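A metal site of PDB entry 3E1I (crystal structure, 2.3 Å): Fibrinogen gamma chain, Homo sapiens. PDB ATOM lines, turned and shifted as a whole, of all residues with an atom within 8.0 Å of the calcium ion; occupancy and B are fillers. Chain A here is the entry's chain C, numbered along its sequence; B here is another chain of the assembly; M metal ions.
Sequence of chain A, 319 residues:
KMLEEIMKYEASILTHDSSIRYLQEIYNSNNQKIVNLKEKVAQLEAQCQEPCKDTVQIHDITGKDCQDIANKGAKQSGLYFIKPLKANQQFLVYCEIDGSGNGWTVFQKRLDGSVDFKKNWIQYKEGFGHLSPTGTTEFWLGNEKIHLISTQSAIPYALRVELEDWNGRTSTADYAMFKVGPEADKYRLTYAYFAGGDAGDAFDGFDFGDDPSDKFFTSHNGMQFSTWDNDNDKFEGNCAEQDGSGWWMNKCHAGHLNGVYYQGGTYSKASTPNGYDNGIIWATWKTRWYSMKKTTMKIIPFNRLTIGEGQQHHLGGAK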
ATOM      1  N   PHE A 206      11.656  23.571  17.142  1.00  0.00           N
ATOM      2  CA  PHE A 206      12.989  24.125  16.923  1.00  0.00           C
ATOM      3  C   PHE A 206      14.099  23.203  17.424  1.00  0.00           C
ATOM      4  O   PHE A 206      13.977  22.553  18.473  1.00  0.00           O
ATOM      5  CB  PHE A 206      13.099  25.544  17.540  1.00  0.00           C
ATOM      6  CG  PHE A 206      14.294  26.325  17.049  1.00  0.00           C
ATOM      7  CD1 PHE A 206      14.246  27.017  15.845  1.00  0.00           C
ATOM      8  CD2 PHE A 206      15.486  26.351  17.785  1.00  0.00           C
ATOM      9  CE1 PHE A 206      15.355  27.728  15.373  1.00  0.00           C
ATOM     10  CE2 PHE A 206      16.606  27.039  17.329  1.00  0.00           C
ATOM     11  CZ  PHE A 206      16.538  27.753  16.119  1.00  0.00           C
ATOM     12  N   ASP A 207      15.181  23.124  16.644  1.00  0.00           N
ATOM     13  CA  ASP A 207      16.389  22.374  17.026  1.00  0.00           C
ATOM     14  C   ASP A 207      17.239  23.226  17.975  1.00  0.00           C
ATOM     15  O   ASP A 207      18.217  23.847  17.556  1.00  0.00           O
ATOM     16  CB  ASP A 207      17.162  21.978  15.751  1.00  0.00           C
ATOM     17  CG  ASP A 207      18.376  21.076  16.014  1.00  0.00           C
ATOM     18  OD1 ASP A 207      19.039  20.698  15.032  1.00  0.00           O
ATOM     19  OD2 ASP A 207      18.688  20.726  17.174  1.00  0.00           O
ATOM     20  N   PHE A 208      16.868  23.232  19.260  1.00  0.00           N
ATOM     21  CA  PHE A 208      17.500  24.104  20.276  1.00  0.00           C
ATOM     22  C   PHE A 208      18.922  23.711  20.657  1.00  0.00           C
ATOM     23  O   PHE A 208      19.753  24.581  20.946  1.00  0.00           O
ATOM     24  CB  PHE A 208      16.664  24.140  21.561  1.00  0.00           C
ATOM     25  CG  PHE A 208      15.351  24.855  21.433  1.00  0.00           C
ATOM     26  CD1 PHE A 208      15.300  26.242  21.324  1.00  0.00           C
ATOM     27  CD2 PHE A 208      14.153  24.140  21.447  1.00  0.00           C
ATOM     28  CE1 PHE A 208      14.070  26.917  21.207  1.00  0.00           C
ATOM     29  CE2 PHE A 208      12.919  24.808  21.334  1.00  0.00           C
ATOM     30  CZ  PHE A 208      12.889  26.203  21.216  1.00  0.00           C
ATOM     31  N   GLY A 209      19.181  22.409  20.715  1.00  0.00           N
ATOM     32  CA  GLY A 209      20.467  21.937  21.202  1.00  0.00           C
ATOM     33  C   GLY A 209      20.795  20.523  20.813  1.00  0.00           C
ATOM     34  O   GLY A 209      20.402  20.065  19.741  1.00  0.00           O
ATOM     35  N   ASP A 210      21.506  19.839  21.703  1.00  0.00           N
ATOM     36  CA  ASP A 210      22.123  18.542  21.414  1.00  0.00           C
ATOM     37  C   ASP A 210      21.150  17.364  21.319  1.00  0.00           C
ATOM     38  O   ASP A 210      21.386  16.405  20.585  1.00  0.00           O
ATOM     39  CB  ASP A 210      23.191  18.229  22.460  1.00  0.00           C
ATOM     40  CG  ASP A 210      24.035  17.049  22.084  1.00  0.00           C
ATOM     41  OD1 ASP A 210      24.400  16.920  20.891  1.00  0.00           O
ATOM     42  OD2 ASP A 210      24.351  16.241  22.978  1.00  0.00           O
ATOM     43  N   ASP A 211      20.094  17.420  22.128  1.00  0.00           N
ATOM     44  CA  ASP A 211      19.052  16.398  22.163  1.00  0.00           C
ATOM     45  C   ASP A 211      18.484  16.226  20.756  1.00  0.00           C
ATOM     46  O   ASP A 211      18.041  17.216  20.152  1.00  0.00           O
ATOM     47  CB  ASP A 211      17.957  16.821  23.138  1.00  0.00           C
ATOM     48  CG  ASP A 211      17.098  15.659  23.610  1.00  0.00           C
ATOM     49  OD1 ASP A 211      16.919  15.523  24.838  1.00  0.00           O
ATOM     50  OD2 ASP A 211      16.593  14.892  22.758  1.00  0.00           O
ATOM     51  N   PRO A 212      18.523  14.991  20.220  1.00  0.00           N
ATOM     52  CA  PRO A 212      18.020  14.719  18.856  1.00  0.00           C
ATOM     53  C   PRO A 212      16.511  14.793  18.727  1.00  0.00           C
ATOM     54  O   PRO A 212      16.005  14.783  17.605  1.00  0.00           O
ATOM     55  CB  PRO A 212      18.484  13.272  18.584  1.00  0.00           C
ATOM     56  CG  PRO A 212      18.700  12.667  19.918  1.00  0.00           C
ATOM     57  CD  PRO A 212      19.059  13.774  20.875  1.00  0.00           C
ATOM     58  N   SER A 213      15.791  14.865  19.836  1.00  0.00           N
ATOM     59  CA  SER A 213      14.330  14.870  19.786  1.00  0.00           C
ATOM     60  C   SER A 213      13.683  16.197  20.185  1.00  0.00           C
ATOM     61  O   SER A 213      12.469  16.266  20.326  1.00  0.00           O
ATOM     62  CB  SER A 213      13.784  13.720  20.660  1.00  0.00           C
ATOM     63  OG  SER A 213      14.129  13.936  22.019  1.00  0.00           O
ATOM     64  N   ASP A 214      14.481  17.263  20.339  1.00  0.00           N
ATOM     65  CA  ASP A 214      13.914  18.538  20.811  1.00  0.00           C
ATOM     66  C   ASP A 214      12.971  19.228  19.822  1.00  0.00           C
ATOM     67  O   ASP A 214      11.962  19.799  20.237  1.00  0.00           O
ATOM     68  CB  ASP A 214      14.997  19.512  21.318  1.00  0.00           C
ATOM     69  CG  ASP A 214      16.110  19.768  20.306  1.00  0.00           C
ATOM     70  OD1 ASP A 214      15.977  19.426  19.110  1.00  0.00           O
ATOM     71  OD2 ASP A 214      17.148  20.316  20.709  1.00  0.00           O
ATOM     72  N   LYS A 215      13.287  19.148  18.535  1.00  0.00           N
ATOM     73  CA  LYS A 215      12.465  19.723  17.465  1.00  0.00           C
ATOM     74  C   LYS A 215      11.120  18.992  17.357  1.00  0.00           C
ATOM     75  O   LYS A 215      10.077  19.644  17.268  1.00  0.00           O
ATOM     76  CB  LYS A 215      13.224  19.688  16.131  1.00  0.00           C
ATOM     77  CG  LYS A 215      12.573  20.460  15.011  1.00  0.00           C
ATOM     78  CD  LYS A 215      13.317  20.188  13.699  1.00  0.00           C
ATOM     79  CE  LYS A 215      12.535  20.706  12.505  1.00  0.00           C
ATOM     80  NZ  LYS A 215      12.798  22.145  12.283  1.00  0.00           N
ATOM     81  N   PHE A 216      11.146  17.669  17.376  1.00  0.00           N
ATOM     82  CA  PHE A 216       9.945  16.820  17.463  1.00  0.00           C
ATOM     83  C   PHE A 216       9.058  17.160  18.668  1.00  0.00           C
ATOM     84  O   PHE A 216       7.832  17.224  18.550  1.00  0.00           O
ATOM     85  CB  PHE A 216      10.334  15.325  17.517  1.00  0.00           C
ATOM     86  CG  PHE A 216       9.156  14.373  17.649  1.00  0.00           C
ATOM     87  CD1 PHE A 216       8.368  14.058  16.531  1.00  0.00           C
ATOM     88  CD2 PHE A 216       8.863  13.764  18.865  1.00  0.00           C
ATOM     89  CE1 PHE A 216       7.277  13.161  16.643  1.00  0.00           C
ATOM     90  CE2 PHE A 216       7.781  12.873  18.996  1.00  0.00           C
ATOM     91  CZ  PHE A 216       6.993  12.572  17.879  1.00  0.00           C
ATOM     92  N   HIS B   2      12.167  22.991  25.079  1.00  0.00           N
ATOM     93  CA  HIS B   2      12.139  21.537  25.261  1.00  0.00           C
ATOM     94  C   HIS B   2      12.262  21.135  26.739  1.00  0.00           C
ATOM     95  O   HIS B   2      12.687  21.945  27.563  1.00  0.00           O
ATOM     96  CB  HIS B   2      13.282  20.947  24.420  1.00  0.00           C
ATOM     97  CG  HIS B   2      13.421  19.468  24.501  1.00  0.00           C
ATOM     98  ND1 HIS B   2      12.338  18.600  24.453  1.00  0.00           N
ATOM     99  CD2 HIS B   2      14.522  18.682  24.594  1.00  0.00           C
ATOM    100  CE1 HIS B   2      12.770  17.354  24.529  1.00  0.00           C
ATOM    101  NE2 HIS B   2      14.095  17.382  24.614  1.00  0.00           N
HETATM  102 CA    CA M   1      18.422  18.972  18.643  1.00  0.00          CA
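OD1 of Asp 211 sits at hydrogen-bond distance from NE2 of His 2 of chain B, at 3.4 Å.
The side-chain carboxylate of Asp 211 sits at hydrogen-bond distance from the side-chain hydroxyl of Ser 213 (2.7 Å).
OD2 of Asp 214 sits close to N of Phe 208 (3.3 Å).
The calcium ion is bound by the side-chain carboxylate (OD2) of Asp 207, the backbone carbonyl oxygen (O) of Asp 211, the backbone carbonyl oxygen (O) of Gly 209, the side-chain carboxylate (OD1) of Asp 214 and the side-chain carboxylate (OD2) of Asp 214.
Of the 12 residues printed, 4 come within 4 Å of the calcium ion.
The nearest printed residue that does not touch the calcium ion is Asp 210 (4.1 Å).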
